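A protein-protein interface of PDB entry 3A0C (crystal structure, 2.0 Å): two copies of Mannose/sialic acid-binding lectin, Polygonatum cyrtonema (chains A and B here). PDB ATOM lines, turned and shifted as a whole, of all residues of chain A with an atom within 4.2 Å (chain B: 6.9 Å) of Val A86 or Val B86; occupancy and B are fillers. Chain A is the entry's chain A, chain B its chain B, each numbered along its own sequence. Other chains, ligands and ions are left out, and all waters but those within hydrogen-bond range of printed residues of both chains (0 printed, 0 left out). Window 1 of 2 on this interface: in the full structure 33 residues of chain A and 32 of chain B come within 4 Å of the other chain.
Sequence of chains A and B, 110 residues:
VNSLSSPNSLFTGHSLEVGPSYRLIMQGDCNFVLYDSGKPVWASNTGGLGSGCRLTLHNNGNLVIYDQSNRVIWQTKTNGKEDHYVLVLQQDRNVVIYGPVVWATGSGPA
The side-chain amide nitrogen (ND2) of Asn B2 lies within hydrogen-bond range of the side-chain hydroxyl (OG) of Ser A3, at 3.2 Å.
N of Ile A97 sits at hydrogen-bond distance from O of Trp B103 (2.8 Å).
The backbone carbonyl oxygen (O) of Val A96 lies within hydrogen-bond range of the backbone NH (N) of Val A88, 2.6 Å away.
O of Val B86 sits at hydrogen-bond distance from N of Tyr B98, 2.9 Å away.
N of Val B88 sits at hydrogen-bond distance from O of Val B96 (2.6 Å).
O of Val A86 is in hydrogen-bond range of N of Tyr A98.
The side-chain hydroxyl (OG) of Ser B6 is in hydrogen-bond range of the backbone NH (N) of Tyr B85 (2.8 Å).
OH of Tyr B98 lies within hydrogen-bond range of OE1 of Gln B90, at 2.7 Å.
Among the printed residues, pairs that only touch across the chains: Tyr A98 with Val B86, Val A96 with Trp B103, Val A86 with Tyr B98, Tyr A98 with His B84, Val A88 with Ser B3, Tyr A98 with Tyr B98, Tyr A98 with Tyr B85, Tyr A98 with Ser B5, Ser A3 with Val B88, Val A86 with Val B86, Tyr A85 with Tyr B98 and Tyr A98 with Gly B99.
Val A86 touches just these residues of chain B: Val B86 (3.7 Å) and Tyr B98 (3.4 Å).
Val B86 touches just these residues of chain A: Val A86 and Tyr A98.
Of the printed residues of chain A, Trp B103 touches Val A96 (3.3 Å) and Ile A97 (2.8 Å).
Of the printed residues of chain A, Asn B2 touches Ser A3.
Printed residues of chain B within 4 Å of Val A88: Ser B3.
Printed residues of chain B within 4 Å of Ile A97: Trp B103 (2.8 Å).
Leu B87 touches none of the printed residues of chain A.
Ile B97 touches none of the printed residues of chain A.
The nearest printed residue of chain A that does not touch Tyr B85 is Val A96 (7.5 Å).
Of the 11 printed residues of chain A, 7 touch a printed residue of chain B.
Printed residues of chain A that touch a printed residue of chain B: Ser A3, Tyr A85, Val A86, Val A88, Val A96, Ile A97 and Tyr A98.
Hydrophobic or aromatic side chains of chain A within 4 Å of the printed part of chain B: Val A86, Val A88, Val A96, Ile A97 and Tyr A98.
Of the 19 printed residues of chain B, 10 touch a printed residue of chain A.
Printed residues of chain B that touch a printed residue of chain A: Asn B2, Ser B3, Ser B5, His B84, Tyr B85, Val B86, Val B88, Tyr B98, Gly B99 and Trp B103.
Hydrophobic or aromatic side chains of chain B that line the printed part of chain A: Val B86, Val B88, Tyr B98 and Trp B103.
Among the printed residues, 14 pairs touch across the chains.
Tyr A85 touches Tyr B98, and with the chains exchanged Tyr A98 touches Tyr B85.
Val A86 touches Tyr B98, and with the chains exchanged Tyr A98 touches Val B86.
Tyr A98 touches Ser B5, but with the chains exchanged Ser A5 does not touch Tyr B98 (4.04 Å).
Tyr A98 touches its own counterpart, Tyr B98.
Positions printed for both chains: 3, 4, 5, 57, 85, 86, 87, 88, 96, 97 and 98.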
ATOM      1  N   SER A   3      19.544  -9.904   8.568  1.00  0.00           N
ATOM      2  CA  SER A   3      19.049  -8.709   9.255  1.00  0.00           C
ATOM      3  C   SER A   3      17.546  -8.776   9.449  1.00  0.00           C
ATOM      4  O   SER A   3      16.842  -9.418   8.682  1.00  0.00           O
ATOM      5  CB  SER A   3      19.388  -7.440   8.461  1.00  0.00           C
ATOM      6  OG  SER A   3      18.502  -7.283   7.369  1.00  0.00           O
ATOM      7  N   LEU A   4      17.070  -8.121  10.495  1.00  0.00           N
ATOM      8  CA  LEU A   4      15.646  -8.059  10.814  1.00  0.00           C
ATOM      9  C   LEU A   4      15.393  -6.608  11.208  1.00  0.00           C
ATOM     10  O   LEU A   4      15.906  -6.142  12.220  1.00  0.00           O
ATOM     11  CB  LEU A   4      15.296  -8.962  12.005  1.00  0.00           C
ATOM     12  CG  LEU A   4      13.824  -8.895  12.444  1.00  0.00           C
ATOM     13  CD1 LEU A   4      13.004  -9.756  11.506  1.00  0.00           C
ATOM     14  CD2 LEU A   4      13.648  -9.372  13.892  1.00  0.00           C
ATOM     15  N   SER A   5      14.609  -5.888  10.421  1.00  0.00           N
ATOM     16  CA  SER A   5      14.360  -4.491  10.731  1.00  0.00           C
ATOM     17  C   SER A   5      12.978  -4.178  11.293  1.00  0.00           C
ATOM     18  O   SER A   5      11.998  -4.826  10.955  1.00  0.00           O
ATOM     19  CB  SER A   5      14.634  -3.630   9.498  1.00  0.00           C
ATOM     20  OG  SER A   5      13.802  -4.012   8.423  1.00  0.00           O
ATOM     21  N   LEU A  57      11.216  -7.011  16.737  1.00  0.00           N
ATOM     22  CA  LEU A  57      12.047  -5.840  17.005  1.00  0.00           C
ATOM     23  C   LEU A  57      11.128  -4.623  16.753  1.00  0.00           C
ATOM     24  O   LEU A  57      10.778  -4.328  15.619  1.00  0.00           O
ATOM     25  CB  LEU A  57      13.270  -5.780  16.075  1.00  0.00           C
ATOM     26  CG  LEU A  57      14.119  -4.498  16.198  1.00  0.00           C
ATOM     27  CD1 LEU A  57      14.630  -4.366  17.610  1.00  0.00           C
ATOM     28  CD2 LEU A  57      15.280  -4.520  15.230  1.00  0.00           C
ATOM     29  N   TYR A  85      14.730   0.647  13.693  1.00  0.00           N
ATOM     30  CA  TYR A  85      15.967  -0.021  14.089  1.00  0.00           C
ATOM     31  C   TYR A  85      16.168  -1.310  13.303  1.00  0.00           C
ATOM     32  O   TYR A  85      15.300  -1.720  12.513  1.00  0.00           O
ATOM     33  CB  TYR A  85      15.936  -0.351  15.585  1.00  0.00           C
ATOM     34  CG  TYR A  85      15.840   0.862  16.471  1.00  0.00           C
ATOM     35  CD1 TYR A  85      14.671   1.631  16.520  1.00  0.00           C
ATOM     36  CD2 TYR A  85      16.931   1.269  17.238  1.00  0.00           C
ATOM     37  CE1 TYR A  85      14.592   2.788  17.314  1.00  0.00           C
ATOM     38  CE2 TYR A  85      16.870   2.422  18.040  1.00  0.00           C
ATOM     39  CZ  TYR A  85      15.697   3.178  18.070  1.00  0.00           C
ATOM     40  OH  TYR A  85      15.632   4.314  18.848  1.00  0.00           O
ATOM     41  N   VAL A  86      17.307  -1.959  13.533  1.00  0.00           N
ATOM     42  CA  VAL A  86      17.628  -3.184  12.819  1.00  0.00           C
ATOM     43  C   VAL A  86      18.417  -4.136  13.727  1.00  0.00           C
ATOM     44  O   VAL A  86      19.218  -3.700  14.552  1.00  0.00           O
ATOM     45  CB  VAL A  86      18.468  -2.863  11.509  1.00  0.00           C
ATOM     46  CG1 VAL A  86      19.867  -2.343  11.878  1.00  0.00           C
ATOM     47  CG2 VAL A  86      18.557  -4.089  10.612  1.00  0.00           C
ATOM     48  N   LEU A  87      18.167  -5.429  13.574  1.00  0.00           N
ATOM     49  CA  LEU A  87      18.848  -6.472  14.331  1.00  0.00           C
ATOM     50  C   LEU A  87      19.760  -7.142  13.300  1.00  0.00           C
ATOM     51  O   LEU A  87      19.271  -7.691  12.309  1.00  0.00           O
ATOM     52  CB  LEU A  87      17.817  -7.472  14.856  1.00  0.00           C
ATOM     53  CG  LEU A  87      18.242  -8.607  15.789  1.00  0.00           C
ATOM     54  CD1 LEU A  87      17.019  -9.443  16.126  1.00  0.00           C
ATOM     55  CD2 LEU A  87      19.278  -9.486  15.135  1.00  0.00           C
ATOM     56  N   VAL A  88      21.070  -7.107  13.529  1.00  0.00           N
ATOM     57  CA  VAL A  88      22.023  -7.682  12.582  1.00  0.00           C
ATOM     58  C   VAL A  88      22.896  -8.840  13.105  1.00  0.00           C
ATOM     59  O   VAL A  88      23.580  -8.714  14.126  1.00  0.00           O
ATOM     60  CB  VAL A  88      22.979  -6.544  12.018  1.00  0.00           C
ATOM     61  CG1 VAL A  88      23.987  -7.107  11.011  1.00  0.00           C
ATOM     62  CG2 VAL A  88      22.151  -5.452  11.381  1.00  0.00           C
ATOM     63  N   VAL A  96      23.881  -7.618  16.786  1.00  0.00           N
ATOM     64  CA  VAL A  96      23.671  -6.246  17.226  1.00  0.00           C
ATOM     65  C   VAL A  96      22.398  -5.550  16.741  1.00  0.00           C
ATOM     66  O   VAL A  96      21.928  -5.771  15.623  1.00  0.00           O
ATOM     67  CB  VAL A  96      24.884  -5.384  16.774  1.00  0.00           C
ATOM     68  CG1 VAL A  96      24.866  -4.037  17.451  1.00  0.00           C
ATOM     69  CG2 VAL A  96      26.176  -6.131  17.050  1.00  0.00           C
ATOM     70  N   ILE A  97      21.858  -4.696  17.607  1.00  0.00           N
ATOM     71  CA  ILE A  97      20.679  -3.890  17.295  1.00  0.00           C
ATOM     72  C   ILE A  97      21.211  -2.467  17.080  1.00  0.00           C
ATOM     73  O   ILE A  97      21.925  -1.923  17.936  1.00  0.00           O
ATOM     74  CB  ILE A  97      19.649  -3.862  18.474  1.00  0.00           C
ATOM     75  CG1 ILE A  97      19.045  -5.252  18.690  1.00  0.00           C
ATOM     76  CG2 ILE A  97      18.539  -2.853  18.196  1.00  0.00           C
ATOM     77  CD1 ILE A  97      17.999  -5.318  19.809  1.00  0.00           C
ATOM     78  N   TYR A  98      20.889  -1.880  15.932  1.00  0.00           N
ATOM     79  CA  TYR A  98      21.323  -0.516  15.626  1.00  0.00           C
ATOM     80  C   TYR A  98      20.122   0.386  15.374  1.00  0.00           C
ATOM     81  O   TYR A  98      19.061  -0.084  14.961  1.00  0.00           O
ATOM     82  CB  TYR A  98      22.217  -0.473  14.370  1.00  0.00           C
ATOM     83  CG  TYR A  98      23.542  -1.215  14.454  1.00  0.00           C
ATOM     84  CD1 TYR A  98      23.653  -2.545  14.019  1.00  0.00           C
ATOM     85  CD2 TYR A  98      24.700  -0.559  14.871  1.00  0.00           C
ATOM     86  CE1 TYR A  98      24.881  -3.188  13.984  1.00  0.00           C
ATOM     87  CE2 TYR A  98      25.933  -1.196  14.840  1.00  0.00           C
ATOM     88  CZ  TYR A  98      26.017  -2.504  14.392  1.00  0.00           C
ATOM     89  OH  TYR A  98      27.249  -3.110  14.313  1.00  0.00           O
ATOM     90  N   ASN B   2      23.921  -9.077   3.677  1.00  0.00           N
ATOM     91  CA  ASN B   2      23.277  -7.860   3.192  1.00  0.00           C
ATOM     92  C   ASN B   2      23.489  -6.695   4.137  1.00  0.00           C
ATOM     93  O   ASN B   2      22.676  -5.784   4.193  1.00  0.00           O
ATOM     94  CB  ASN B   2      21.779  -8.064   2.941  1.00  0.00           C
ATOM     95  CG  ASN B   2      21.027  -8.425   4.182  1.00  0.00           C
ATOM     96  OD1 ASN B   2      21.036  -9.569   4.598  1.00  0.00           O
ATOM     97  ND2 ASN B   2      20.374  -7.454   4.788  1.00  0.00           N
ATOM     98  N   SER B   3      24.602  -6.726   4.866  1.00  0.00           N
ATOM     99  CA  SER B   3      24.945  -5.674   5.815  1.00  0.00           C
ATOM    100  C   SER B   3      26.457  -5.421   5.848  1.00  0.00           C
ATOM    101  O   SER B   3      27.247  -6.328   5.593  1.00  0.00           O
ATOM    102  CB  SER B   3      24.466  -6.064   7.216  1.00  0.00           C
ATOM    103  OG  SER B   3      25.279  -7.073   7.781  1.00  0.00           O
ATOM    104  N   LEU B   4      26.835  -4.181   6.150  1.00  0.00           N
ATOM    105  CA  LEU B   4      28.229  -3.765   6.254  1.00  0.00           C
ATOM    106  C   LEU B   4      28.274  -2.936   7.536  1.00  0.00           C
ATOM    107  O   LEU B   4      27.641  -1.886   7.612  1.00  0.00           O
ATOM    108  CB  LEU B   4      28.623  -2.875   5.068  1.00  0.00           C
ATOM    109  CG  LEU B   4      30.049  -2.300   5.126  1.00  0.00           C
ATOM    110  CD1 LEU B   4      31.023  -3.396   4.726  1.00  0.00           C
ATOM    111  CD2 LEU B   4      30.186  -1.089   4.219  1.00  0.00           C
ATOM    112  N   SER B   5      29.008  -3.383   8.545  1.00  0.00           N
ATOM    113  CA  SER B   5      29.059  -2.622   9.796  1.00  0.00           C
ATOM    114  C   SER B   5      30.384  -1.908  10.053  1.00  0.00           C
ATOM    115  O   SER B   5      31.430  -2.374   9.639  1.00  0.00           O
ATOM    116  CB  SER B   5      28.741  -3.540  10.956  1.00  0.00           C
ATOM    117  OG  SER B   5      29.709  -4.558  11.008  1.00  0.00           O
ATOM    118  N   SER B   6      30.311  -0.776  10.749  1.00  0.00           N
ATOM    119  CA  SER B   6      31.461   0.070  11.089  1.00  0.00           C
ATOM    120  C   SER B   6      32.607  -0.696  11.715  1.00  0.00           C
ATOM    121  O   SER B   6      32.382  -1.483  12.612  1.00  0.00           O
ATOM    122  CB  SER B   6      31.031   1.138  12.097  1.00  0.00           C
ATOM    123  OG  SER B   6      29.861   1.782  11.670  1.00  0.00           O
ATOM    124  N   LEU B  57      32.237   2.565   5.829  1.00  0.00           N
ATOM    125  CA  LEU B  57      31.257   3.107   6.764  1.00  0.00           C
ATOM    126  C   LEU B  57      32.045   3.306   8.065  1.00  0.00           C
ATOM    127  O   LEU B  57      32.440   2.330   8.700  1.00  0.00           O
ATOM    128  CB  LEU B  57      30.103   2.121   6.991  1.00  0.00           C
ATOM    129  CG  LEU B  57      29.106   2.546   8.083  1.00  0.00           C
ATOM    130  CD1 LEU B  57      28.551   3.929   7.767  1.00  0.00           C
ATOM    131  CD2 LEU B  57      27.985   1.519   8.203  1.00  0.00           C
ATOM    132  N   HIS B  58      32.303   4.556   8.442  1.00  0.00           N
ATOM    133  CA  HIS B  58      33.057   4.858   9.658  1.00  0.00           C
ATOM    134  C   HIS B  58      32.225   4.674  10.918  1.00  0.00           C
ATOM    135  O   HIS B  58      30.994   4.612  10.857  1.00  0.00           O
ATOM    136  CB  HIS B  58      33.584   6.295   9.614  1.00  0.00           C
ATOM    137  CG  HIS B  58      34.538   6.540   8.500  1.00  0.00           C
ATOM    138  ND1 HIS B  58      35.774   5.934   8.437  1.00  0.00           N
ATOM    139  CD2 HIS B  58      34.413   7.266   7.367  1.00  0.00           C
ATOM    140  CE1 HIS B  58      36.370   6.272   7.307  1.00  0.00           C
ATOM    141  NE2 HIS B  58      35.565   7.078   6.639  1.00  0.00           N
ATOM    142  N   GLY B  61      29.144   6.995  11.656  1.00  0.00           N
ATOM    143  CA  GLY B  61      27.975   6.988  10.796  1.00  0.00           C
ATOM    144  C   GLY B  61      28.144   7.570   9.407  1.00  0.00           C
ATOM    145  O   GLY B  61      27.196   7.569   8.625  1.00  0.00           O
ATOM    146  N   HIS B  84      29.268   2.786  16.772  1.00  0.00           N
ATOM    147  CA  HIS B  84      29.288   1.727  15.766  1.00  0.00           C
ATOM    148  C   HIS B  84      27.957   1.803  15.033  1.00  0.00           C
ATOM    149  O   HIS B  84      26.906   1.988  15.651  1.00  0.00           O
ATOM    150  CB  HIS B  84      29.470   0.350  16.403  1.00  0.00           C
ATOM    151  CG  HIS B  84      30.864   0.090  16.869  1.00  0.00           C
ATOM    152  ND1 HIS B  84      31.922  -0.038  15.998  1.00  0.00           N
ATOM    153  CD2 HIS B  84      31.383  -0.036  18.111  1.00  0.00           C
ATOM    154  CE1 HIS B  84      33.034  -0.231  16.682  1.00  0.00           C
ATOM    155  NE2 HIS B  84      32.734  -0.235  17.967  1.00  0.00           N
ATOM    156  N   TYR B  85      28.018   1.703  13.710  1.00  0.00           N
ATOM    157  CA  TYR B  85      26.836   1.787  12.858  1.00  0.00           C
ATOM    158  C   TYR B  85      26.818   0.644  11.861  1.00  0.00           C
ATOM    159  O   TYR B  85      27.757  -0.130  11.787  1.00  0.00           O
ATOM    160  CB  TYR B  85      26.828   3.106  12.085  1.00  0.00           C
ATOM    161  CG  TYR B  85      26.752   4.338  12.958  1.00  0.00           C
ATOM    162  CD1 TYR B  85      27.846   4.756  13.725  1.00  0.00           C
ATOM    163  CD2 TYR B  85      25.571   5.072  13.036  1.00  0.00           C
ATOM    164  CE1 TYR B  85      27.752   5.875  14.545  1.00  0.00           C
ATOM    165  CE2 TYR B  85      25.470   6.188  13.851  1.00  0.00           C
ATOM    166  CZ  TYR B  85      26.558   6.582  14.599  1.00  0.00           C
ATOM    167  OH  TYR B  85      26.423   7.680  15.409  1.00  0.00           O
ATOM    168  N   VAL B  86      25.752   0.566  11.077  1.00  0.00           N
ATOM    169  CA  VAL B  86      25.609  -0.499  10.085  1.00  0.00           C
ATOM    170  C   VAL B  86      24.901   0.012   8.814  1.00  0.00           C
ATOM    171  O   VAL B  86      24.034   0.890   8.870  1.00  0.00           O
ATOM    172  CB  VAL B  86      24.811  -1.729  10.686  1.00  0.00           C
ATOM    173  CG1 VAL B  86      23.346  -1.347  10.931  1.00  0.00           C
ATOM    174  CG2 VAL B  86      24.910  -2.941   9.762  1.00  0.00           C
ATOM    175  N   LEU B  87      25.308  -0.529   7.672  1.00  0.00           N
ATOM    176  CA  LEU B  87      24.710  -0.192   6.384  1.00  0.00           C
ATOM    177  C   LEU B  87      23.907  -1.441   5.990  1.00  0.00           C
ATOM    178  O   LEU B  87      24.477  -2.513   5.827  1.00  0.00           O
ATOM    179  CB  LEU B  87      25.816   0.078   5.356  1.00  0.00           C
ATOM    180  CG  LEU B  87      25.490   0.630   3.960  1.00  0.00           C
ATOM    181  CD1 LEU B  87      26.786   0.831   3.194  1.00  0.00           C
ATOM    182  CD2 LEU B  87      24.612  -0.313   3.206  1.00  0.00           C
ATOM    183  N   VAL B  88      22.593  -1.303   5.844  1.00  0.00           N
ATOM    184  CA  VAL B  88      21.752  -2.448   5.491  1.00  0.00           C
ATOM    185  C   VAL B  88      20.950  -2.394   4.180  1.00  0.00           C
ATOM    186  O   VAL B  88      20.120  -1.501   3.973  1.00  0.00           O
ATOM    187  CB  VAL B  88      20.736  -2.767   6.630  1.00  0.00           C
ATOM    188  CG1 VAL B  88      19.948  -4.022   6.297  1.00  0.00           C
ATOM    189  CG2 VAL B  88      21.462  -2.955   7.946  1.00  0.00           C
ATOM    190  N   GLN B  90      18.094  -3.761   2.472  1.00  0.00           N
ATOM    191  CA  GLN B  90      16.865  -4.413   2.908  1.00  0.00           C
ATOM    192  C   GLN B  90      16.033  -5.099   1.830  1.00  0.00           C
ATOM    193  O   GLN B  90      16.096  -4.741   0.659  1.00  0.00           O
ATOM    194  CB  GLN B  90      15.999  -3.392   3.644  1.00  0.00           C
ATOM    195  CG  GLN B  90      16.692  -2.806   4.821  1.00  0.00           C
ATOM    196  CD  GLN B  90      15.898  -1.720   5.485  1.00  0.00           C
ATOM    197  OE1 GLN B  90      16.206  -1.306   6.602  1.00  0.00           O
ATOM    198  NE2 GLN B  90      14.878  -1.231   4.802  1.00  0.00           N
ATOM    199  N   VAL B  96      19.742   1.383   4.047  1.00  0.00           N
ATOM    200  CA  VAL B  96      19.777   2.256   5.211  1.00  0.00           C
ATOM    201  C   VAL B  96      20.995   2.148   6.116  1.00  0.00           C
ATOM    202  O   VAL B  96      21.580   1.073   6.260  1.00  0.00           O
ATOM    203  CB  VAL B  96      18.533   1.976   6.110  1.00  0.00           C
ATOM    204  CG1 VAL B  96      18.402   3.059   7.173  1.00  0.00           C
ATOM    205  CG2 VAL B  96      17.279   1.849   5.258  1.00  0.00           C
ATOM    206  N   ILE B  97      21.355   3.275   6.729  1.00  0.00           N
ATOM    207  CA  ILE B  97      22.438   3.325   7.711  1.00  0.00           C
ATOM    208  C   ILE B  97      21.745   3.512   9.083  1.00  0.00           C
ATOM    209  O   ILE B  97      20.944   4.448   9.252  1.00  0.00           O
ATOM    210  CB  ILE B  97      23.401   4.523   7.478  1.00  0.00           C
ATOM    211  CG1 ILE B  97      24.176   4.327   6.177  1.00  0.00           C
ATOM    212  CG2 ILE B  97      24.377   4.643   8.630  1.00  0.00           C
ATOM    213  CD1 ILE B  97      25.213   5.412   5.912  1.00  0.00           C
ATOM    214  N   TYR B  98      22.027   2.607  10.029  1.00  0.00           N
ATOM    215  CA  TYR B  98      21.463   2.668  11.384  1.00  0.00           C
ATOM    216  C   TYR B  98      22.579   2.818  12.425  1.00  0.00           C
ATOM    217  O   TYR B  98      23.708   2.394  12.193  1.00  0.00           O
ATOM    218  CB  TYR B  98      20.685   1.402  11.729  1.00  0.00           C
ATOM    219  CG  TYR B  98      19.451   1.126  10.910  1.00  0.00           C
ATOM    220  CD1 TYR B  98      19.503   0.308   9.780  1.00  0.00           C
ATOM    221  CD2 TYR B  98      18.208   1.613  11.311  1.00  0.00           C
ATOM    222  CE1 TYR B  98      18.345  -0.025   9.075  1.00  0.00           C
ATOM    223  CE2 TYR B  98      17.040   1.282  10.609  1.00  0.00           C
ATOM    224  CZ  TYR B  98      17.114   0.465   9.498  1.00  0.00           C
ATOM    225  OH  TYR B  98      15.947   0.138   8.839  1.00  0.00           O
ATOM    226  N   GLY B  99      22.251   3.411  13.572  1.00  0.00           N
ATOM    227  CA  GLY B  99      23.239   3.588  14.626  1.00  0.00           C
ATOM    228  C   GLY B  99      22.869   4.696  15.593  1.00  0.00           C
ATOM    229  O   GLY B  99      21.988   5.501  15.282  1.00  0.00           O
ATOM    230  N   TRP B 103      21.937  -2.468  21.461  1.00  0.00           N
ATOM    231  CA  TRP B 103      22.069  -3.709  22.207  1.00  0.00           C
ATOM    232  C   TRP B 103      22.848  -4.710  21.355  1.00  0.00           C
ATOM    233  O   TRP B 103      22.944  -4.547  20.141  1.00  0.00           O
ATOM    234  CB  TRP B 103      20.671  -4.252  22.524  1.00  0.00           C
ATOM    235  CG  TRP B 103      20.638  -5.517  23.369  1.00  0.00           C
ATOM    236  CD1 TRP B 103      20.677  -5.607  24.733  1.00  0.00           C
ATOM    237  CD2 TRP B 103      20.519  -6.854  22.883  1.00  0.00           C
ATOM    238  NE1 TRP B 103      20.583  -6.917  25.123  1.00  0.00           N
ATOM    239  CE2 TRP B 103      20.482  -7.707  24.007  1.00  0.00           C
ATOM    240  CE3 TRP B 103      20.433  -7.417  21.603  1.00  0.00           C
ATOM    241  CZ2 TRP B 103      20.358  -9.099  23.890  1.00  0.00           C
ATOM    242  CZ3 TRP B 103      20.309  -8.793  21.490  1.00  0.00           C
ATOM    243  CH2 TRP B 103      20.271  -9.616  22.626  1.00  0.00           C
